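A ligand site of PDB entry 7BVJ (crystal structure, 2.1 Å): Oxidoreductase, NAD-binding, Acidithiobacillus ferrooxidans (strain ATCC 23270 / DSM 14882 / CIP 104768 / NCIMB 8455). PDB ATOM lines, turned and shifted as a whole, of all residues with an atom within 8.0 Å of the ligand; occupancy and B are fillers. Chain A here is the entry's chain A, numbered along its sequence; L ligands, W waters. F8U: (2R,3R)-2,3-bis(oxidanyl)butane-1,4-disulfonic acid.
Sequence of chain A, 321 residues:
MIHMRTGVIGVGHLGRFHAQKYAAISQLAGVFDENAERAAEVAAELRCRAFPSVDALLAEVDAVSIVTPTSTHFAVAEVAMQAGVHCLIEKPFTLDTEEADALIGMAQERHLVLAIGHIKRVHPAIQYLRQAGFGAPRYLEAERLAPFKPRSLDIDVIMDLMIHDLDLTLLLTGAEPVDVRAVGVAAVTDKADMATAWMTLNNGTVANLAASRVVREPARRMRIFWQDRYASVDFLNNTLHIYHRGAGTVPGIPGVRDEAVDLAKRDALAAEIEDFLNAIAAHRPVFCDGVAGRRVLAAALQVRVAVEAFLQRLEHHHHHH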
ATOM      1  N   TYR A 139       0.222   4.308   8.631  1.00  0.00           N
ATOM      2  CA  TYR A 139       1.487   4.412   9.353  1.00  0.00           C
ATOM      3  C   TYR A 139       2.349   3.189   9.081  1.00  0.00           C
ATOM      4  O   TYR A 139       1.841   2.063   9.061  1.00  0.00           O
ATOM      5  CB  TYR A 139       1.203   4.575  10.856  1.00  0.00           C
ATOM      6  CG  TYR A 139       2.403   4.623  11.774  1.00  0.00           C
ATOM      7  CD1 TYR A 139       3.373   5.605  11.642  1.00  0.00           C
ATOM      8  CD2 TYR A 139       2.544   3.706  12.809  1.00  0.00           C
ATOM      9  CE1 TYR A 139       4.463   5.652  12.495  1.00  0.00           C
ATOM     10  CE2 TYR A 139       3.621   3.745  13.647  1.00  0.00           C
ATOM     11  CZ  TYR A 139       4.577   4.717  13.500  1.00  0.00           C
ATOM     12  OH  TYR A 139       5.644   4.749  14.372  1.00  0.00           O
ATOM     13  N   GLU A 141       6.150   1.435  10.431  1.00  0.00           N
ATOM     14  CA  GLU A 141       7.215   1.437  11.423  1.00  0.00           C
ATOM     15  C   GLU A 141       8.150   0.284  11.073  1.00  0.00           C
ATOM     16  O   GLU A 141       7.708  -0.870  11.049  1.00  0.00           O
ATOM     17  CB  GLU A 141       6.628   1.230  12.818  1.00  0.00           C
ATOM     18  CG  GLU A 141       7.263   1.994  13.911  1.00  0.00           C
ATOM     19  CD  GLU A 141       6.455   1.911  15.202  1.00  0.00           C
ATOM     20  OE1 GLU A 141       6.081   0.787  15.606  1.00  0.00           O
ATOM     21  OE2 GLU A 141       6.209   2.967  15.804  1.00  0.00           O
ATOM     22  N   GLU A 143      12.271  -1.636  11.131  1.00  0.00           N
ATOM     23  CA  GLU A 143      13.629  -1.788  11.653  1.00  0.00           C
ATOM     24  C   GLU A 143      14.441  -2.688  10.734  1.00  0.00           C
ATOM     25  O   GLU A 143      14.027  -3.812  10.424  1.00  0.00           O
ATOM     26  CB  GLU A 143      13.632  -2.373  13.073  1.00  0.00           C
ATOM     27  CG  GLU A 143      12.797  -1.605  14.073  1.00  0.00           C
ATOM     28  CD  GLU A 143      12.470  -2.439  15.297  1.00  0.00           C
ATOM     29  OE1 GLU A 143      13.289  -2.426  16.258  1.00  0.00           O
ATOM     30  OE2 GLU A 143      11.414  -3.100  15.281  1.00  0.00           O
ATOM     31  N   ARG A 221      12.211  -6.133  10.366  1.00  0.00           N
ATOM     32  CA  ARG A 221      10.801  -6.161  10.714  1.00  0.00           C
ATOM     33  C   ARG A 221      10.099  -4.900  10.210  1.00  0.00           C
ATOM     34  O   ARG A 221      10.740  -3.852  10.018  1.00  0.00           O
ATOM     35  CB  ARG A 221      10.630  -6.343  12.219  1.00  0.00           C
ATOM     36  CG  ARG A 221      11.190  -7.697  12.705  1.00  0.00           C
ATOM     37  CD  ARG A 221      10.821  -7.998  14.153  1.00  0.00           C
ATOM     38  NE  ARG A 221      11.031  -6.849  15.035  1.00  0.00           N
ATOM     39  CZ  ARG A 221      12.060  -6.718  15.868  1.00  0.00           C
ATOM     40  NH1 ARG A 221      12.986  -7.658  15.947  1.00  0.00           N
ATOM     41  NH2 ARG A 221      12.144  -5.632  16.632  1.00  0.00           N
ATOM     42  N   MET A 222       8.789  -5.029   9.968  1.00  0.00           N
ATOM     43  CA  MET A 222       7.950  -3.903   9.587  1.00  0.00           C
ATOM     44  C   MET A 222       6.543  -4.103  10.130  1.00  0.00           C
ATOM     45  O   MET A 222       5.895  -5.109   9.820  1.00  0.00           O
ATOM     46  CB  MET A 222       7.889  -3.701   8.066  1.00  0.00           C
ATOM     47  CG  MET A 222       7.035  -2.482   7.649  1.00  0.00           C
ATOM     48  SD  MET A 222       6.983  -2.208   5.862  1.00  0.00           S
ATOM     49  CE  MET A 222       8.532  -1.378   5.627  1.00  0.00           C
ATOM     50  N   ARG A 223       6.075  -3.144  10.905  1.00  0.00           N
ATOM     51  CA  ARG A 223       4.684  -3.077  11.304  1.00  0.00           C
ATOM     52  C   ARG A 223       3.976  -2.017  10.465  1.00  0.00           C
ATOM     53  O   ARG A 223       4.551  -0.963  10.143  1.00  0.00           O
ATOM     54  CB  ARG A 223       4.575  -2.794  12.803  1.00  0.00           C
ATOM     55  CG  ARG A 223       5.025  -4.004  13.628  1.00  0.00           C
ATOM     56  CD  ARG A 223       5.245  -3.691  15.109  1.00  0.00           C
ATOM     57  NE  ARG A 223       6.291  -2.693  15.331  1.00  0.00           N
ATOM     58  CZ  ARG A 223       7.604  -2.938  15.295  1.00  0.00           C
ATOM     59  NH1 ARG A 223       8.080  -4.152  15.044  1.00  0.00           N
ATOM     60  NH2 ARG A 223       8.443  -1.944  15.513  1.00  0.00           N
ATOM     61  N   ILE A 224       2.756  -2.339  10.041  1.00  0.00           N
ATOM     62  CA  ILE A 224       2.009  -1.530   9.090  1.00  0.00           C
ATOM     63  C   ILE A 224       0.589  -1.352   9.629  1.00  0.00           C
ATOM     64  O   ILE A 224      -0.049  -2.328  10.030  1.00  0.00           O
ATOM     65  CB  ILE A 224       1.981  -2.199   7.704  1.00  0.00           C
ATOM     66  CG1 ILE A 224       3.400  -2.632   7.287  1.00  0.00           C
ATOM     67  CG2 ILE A 224       1.344  -1.290   6.703  1.00  0.00           C
ATOM     68  CD1 ILE A 224       3.463  -3.242   5.909  1.00  0.00           C
ATOM     69  N   PHE A 225       0.120  -0.113   9.657  1.00  0.00           N
ATOM     70  CA  PHE A 225      -1.162   0.251  10.243  1.00  0.00           C
ATOM     71  C   PHE A 225      -2.053   0.890   9.188  1.00  0.00           C
ATOM     72  O   PHE A 225      -1.713   1.934   8.610  1.00  0.00           O
ATOM     73  CB  PHE A 225      -0.994   1.217  11.424  1.00  0.00           C
ATOM     74  CG  PHE A 225      -0.151   0.687  12.552  1.00  0.00           C
ATOM     75  CD1 PHE A 225      -0.737   0.233  13.720  1.00  0.00           C
ATOM     76  CD2 PHE A 225       1.251   0.667  12.449  1.00  0.00           C
ATOM     77  CE1 PHE A 225       0.056  -0.253  14.768  1.00  0.00           C
ATOM     78  CE2 PHE A 225       2.035   0.179  13.493  1.00  0.00           C
ATOM     79  CZ  PHE A 225       1.429  -0.272  14.651  1.00  0.00           C
ATOM     80  N   TYR A 230      -3.759  -4.346  11.169  1.00  0.00           N
ATOM     81  CA  TYR A 230      -2.372  -4.237  11.579  1.00  0.00           C
ATOM     82  C   TYR A 230      -1.595  -5.413  11.015  1.00  0.00           C
ATOM     83  O   TYR A 230      -1.917  -6.565  11.327  1.00  0.00           O
ATOM     84  CB  TYR A 230      -2.281  -4.175  13.106  1.00  0.00           C
ATOM     85  CG  TYR A 230      -0.973  -4.572  13.757  1.00  0.00           C
ATOM     86  CD1 TYR A 230      -0.784  -5.861  14.236  1.00  0.00           C
ATOM     87  CD2 TYR A 230       0.032  -3.642  13.965  1.00  0.00           C
ATOM     88  CE1 TYR A 230       0.385  -6.224  14.876  1.00  0.00           C
ATOM     89  CE2 TYR A 230       1.218  -3.991  14.608  1.00  0.00           C
ATOM     90  CZ  TYR A 230       1.385  -5.292  15.069  1.00  0.00           C
ATOM     91  OH  TYR A 230       2.545  -5.657  15.705  1.00  0.00           O
ATOM     92  N   ALA A 231      -0.593  -5.151  10.197  1.00  0.00           N
ATOM     93  CA  ALA A 231       0.262  -6.183   9.634  1.00  0.00           C
ATOM     94  C   ALA A 231       1.642  -6.121  10.287  1.00  0.00           C
ATOM     95  O   ALA A 231       2.263  -5.056  10.318  1.00  0.00           O
ATOM     96  CB  ALA A 231       0.381  -6.035   8.118  1.00  0.00           C
ATOM     97  N   SER A 232       2.118  -7.252  10.790  1.00  0.00           N
ATOM     98  CA  SER A 232       3.466  -7.380  11.320  1.00  0.00           C
ATOM     99  C   SER A 232       4.223  -8.359  10.434  1.00  0.00           C
ATOM    100  O   SER A 232       3.774  -9.491  10.229  1.00  0.00           O
ATOM    101  CB  SER A 232       3.439  -7.838  12.777  1.00  0.00           C
ATOM    102  OG  SER A 232       4.727  -7.804  13.374  1.00  0.00           O
ATOM    103  N   VAL A 233       5.351  -7.915   9.884  1.00  0.00           N
ATOM    104  CA  VAL A 233       6.160  -8.685   8.956  1.00  0.00           C
ATOM    105  C   VAL A 233       7.534  -8.882   9.564  1.00  0.00           C
ATOM    106  O   VAL A 233       8.213  -7.904   9.902  1.00  0.00           O
ATOM    107  CB  VAL A 233       6.274  -7.976   7.599  1.00  0.00           C
ATOM    108  CG1 VAL A 233       7.144  -8.799   6.639  1.00  0.00           C
ATOM    109  CG2 VAL A 233       4.919  -7.731   6.990  1.00  0.00           C
ATOM    110  N   ASP A 234       7.937 -10.145   9.706  1.00  0.00           N
ATOM    111  CA  ASP A 234       9.321 -10.529   9.982  1.00  0.00           C
ATOM    112  C   ASP A 234       9.912 -10.980   8.662  1.00  0.00           C
ATOM    113  O   ASP A 234       9.682 -12.115   8.219  1.00  0.00           O
ATOM    114  CB  ASP A 234       9.393 -11.630  11.027  1.00  0.00           C
ATOM    115  CG  ASP A 234      10.794 -11.844  11.573  1.00  0.00           C
ATOM    116  OD1 ASP A 234      11.829 -11.593  10.859  1.00  0.00           O
ATOM    117  OD2 ASP A 234      10.859 -12.282  12.732  1.00  0.00           O
ATOM    118  N   THR A 239       7.682 -14.365   8.123  1.00  0.00           N
ATOM    119  CA  THR A 239       6.361 -14.505   8.744  1.00  0.00           C
ATOM    120  C   THR A 239       5.541 -13.237   8.621  1.00  0.00           C
ATOM    121  O   THR A 239       6.089 -12.123   8.631  1.00  0.00           O
ATOM    122  CB  THR A 239       6.457 -14.889  10.229  1.00  0.00           C
ATOM    123  OG1 THR A 239       7.094 -13.835  10.956  1.00  0.00           O
ATOM    124  CG2 THR A 239       7.240 -16.185  10.417  1.00  0.00           C
ATOM    125  N   HIS A 241       1.690 -11.502  10.046  1.00  0.00           N
ATOM    126  CA  HIS A 241       0.521 -11.560  10.909  1.00  0.00           C
ATOM    127  C   HIS A 241      -0.359 -10.349  10.663  1.00  0.00           C
ATOM    128  O   HIS A 241       0.140  -9.232  10.623  1.00  0.00           O
ATOM    129  CB  HIS A 241       0.910 -11.622  12.387  1.00  0.00           C
ATOM    130  CG  HIS A 241       1.418 -12.955  12.814  1.00  0.00           C
ATOM    131  ND1 HIS A 241       0.607 -13.917  13.376  1.00  0.00           N
ATOM    132  CD2 HIS A 241       2.650 -13.504  12.704  1.00  0.00           C
ATOM    133  CE1 HIS A 241       1.334 -14.995  13.632  1.00  0.00           C
ATOM    134  NE2 HIS A 241       2.566 -14.774  13.220  1.00  0.00           N
ATOM    135  N   TYR A 243      -3.866  -8.438  12.000  1.00  0.00           N
ATOM    136  CA  TYR A 243      -4.877  -8.320  13.044  1.00  0.00           C
ATOM    137  C   TYR A 243      -6.017  -7.475  12.507  1.00  0.00           C
ATOM    138  O   TYR A 243      -5.788  -6.408  11.911  1.00  0.00           O
ATOM    139  CB  TYR A 243      -4.311  -7.688  14.316  1.00  0.00           C
ATOM    140  CG  TYR A 243      -3.159  -8.423  15.003  1.00  0.00           C
ATOM    141  CD1 TYR A 243      -2.472  -9.459  14.358  1.00  0.00           C
ATOM    142  CD2 TYR A 243      -2.746  -8.063  16.283  1.00  0.00           C
ATOM    143  CE1 TYR A 243      -1.417 -10.116  14.976  1.00  0.00           C
ATOM    144  CE2 TYR A 243      -1.694  -8.726  16.913  1.00  0.00           C
ATOM    145  CZ  TYR A 243      -1.028  -9.750  16.253  1.00  0.00           C
ATOM    146  OH  TYR A 243       0.023 -10.433  16.843  1.00  0.00           O
ATOM    147  N   ILE A 253      -4.665  -7.768  23.954  1.00  0.00           N
ATOM    148  CA  ILE A 253      -5.363  -6.918  22.985  1.00  0.00           C
ATOM    149  C   ILE A 253      -6.775  -7.452  22.811  1.00  0.00           C
ATOM    150  O   ILE A 253      -6.979  -8.451  22.093  1.00  0.00           O
ATOM    151  CB  ILE A 253      -4.631  -6.840  21.634  1.00  0.00           C
ATOM    152  CG1 ILE A 253      -3.166  -6.429  21.794  1.00  0.00           C
ATOM    153  CG2 ILE A 253      -5.341  -5.875  20.694  1.00  0.00           C
ATOM    154  CD1 ILE A 253      -2.239  -7.556  22.086  1.00  0.00           C
ATOM    155  N   ASP A 258      -6.063 -12.361  15.226  1.00  0.00           N
ATOM    156  CA  ASP A 258      -4.735 -12.437  14.644  1.00  0.00           C
ATOM    157  C   ASP A 258      -4.729 -13.591  13.655  1.00  0.00           C
ATOM    158  O   ASP A 258      -4.932 -14.740  14.035  1.00  0.00           O
ATOM    159  CB  ASP A 258      -3.686 -12.629  15.749  1.00  0.00           C
ATOM    160  CG  ASP A 258      -2.402 -13.237  15.235  1.00  0.00           C
ATOM    161  OD1 ASP A 258      -1.794 -14.031  15.979  1.00  0.00           O
ATOM    162  OD2 ASP A 258      -1.978 -12.917  14.106  1.00  0.00           O
HETATM  163  C01 F8U L   1       6.354  -3.813  18.825  1.00  0.00           C
HETATM  164  C02 F8U L   1       6.656  -5.163  19.470  1.00  0.00           C
HETATM  165  C03 F8U L   1       6.283  -6.453  18.726  1.00  0.00           C
HETATM  166  C04 F8U L   1       5.205  -6.358  17.661  1.00  0.00           C
HETATM  167  O06 F8U L   1       5.125  -9.190  17.653  1.00  0.00           O
HETATM  168  O07 F8U L   1       3.359  -8.124  16.650  1.00  0.00           O
HETATM  169  O08 F8U L   1       5.617  -8.120  15.689  1.00  0.00           O
HETATM  170  O09 F8U L   1       5.821  -7.343  19.667  1.00  0.00           O
HETATM  171  O10 F8U L   1       8.024  -5.280  19.633  1.00  0.00           O
HETATM  172  O12 F8U L   1       4.338  -2.310  20.071  1.00  0.00           O
HETATM  173  O13 F8U L   1       4.076  -2.522  17.830  1.00  0.00           O
HETATM  174  O14 F8U L   1       3.836  -4.577  19.176  1.00  0.00           O
HETATM  175  S05 F8U L   1       4.818  -7.961  16.879  1.00  0.00           S
HETATM  176  S11 F8U L   1       4.613  -3.303  19.001  1.00  0.00           S
HETATM  177  O   HOH W   1       4.778   0.486  18.474  1.00  0.00           O
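An oxygen (O08) of the ligand lies within hydrogen-bond range of the side-chain hydroxyl (OG) of Ser 232 (2.5 Å).
An oxygen (O07) of the ligand lies within hydrogen-bond range of the side-chain hydroxyl of Tyr 230 (2.8 Å).
The guanidinium group (NE) of Arg 223 is in salt-bridge range of an oxygen (O13) of the ligand, 3.3 Å away.
The backbone NH of Ser 232 is in hydrogen-bond range of the backbone carbonyl oxygen of His 241 (2.8 Å).
The backbone NH (N) of Tyr 243 lies within hydrogen-bond range of the backbone carbonyl oxygen (O) of Tyr 230, at 2.8 Å.
OE1 of Glu 141 is in salt-bridge range of NE of Arg 223.
The side-chain carboxylate of Glu 143 lies within salt-bridge range of the guanidinium group of Arg 223 (3.2 Å).
Water W1 bridges O13 of the ligand and OE1 of Glu 141.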
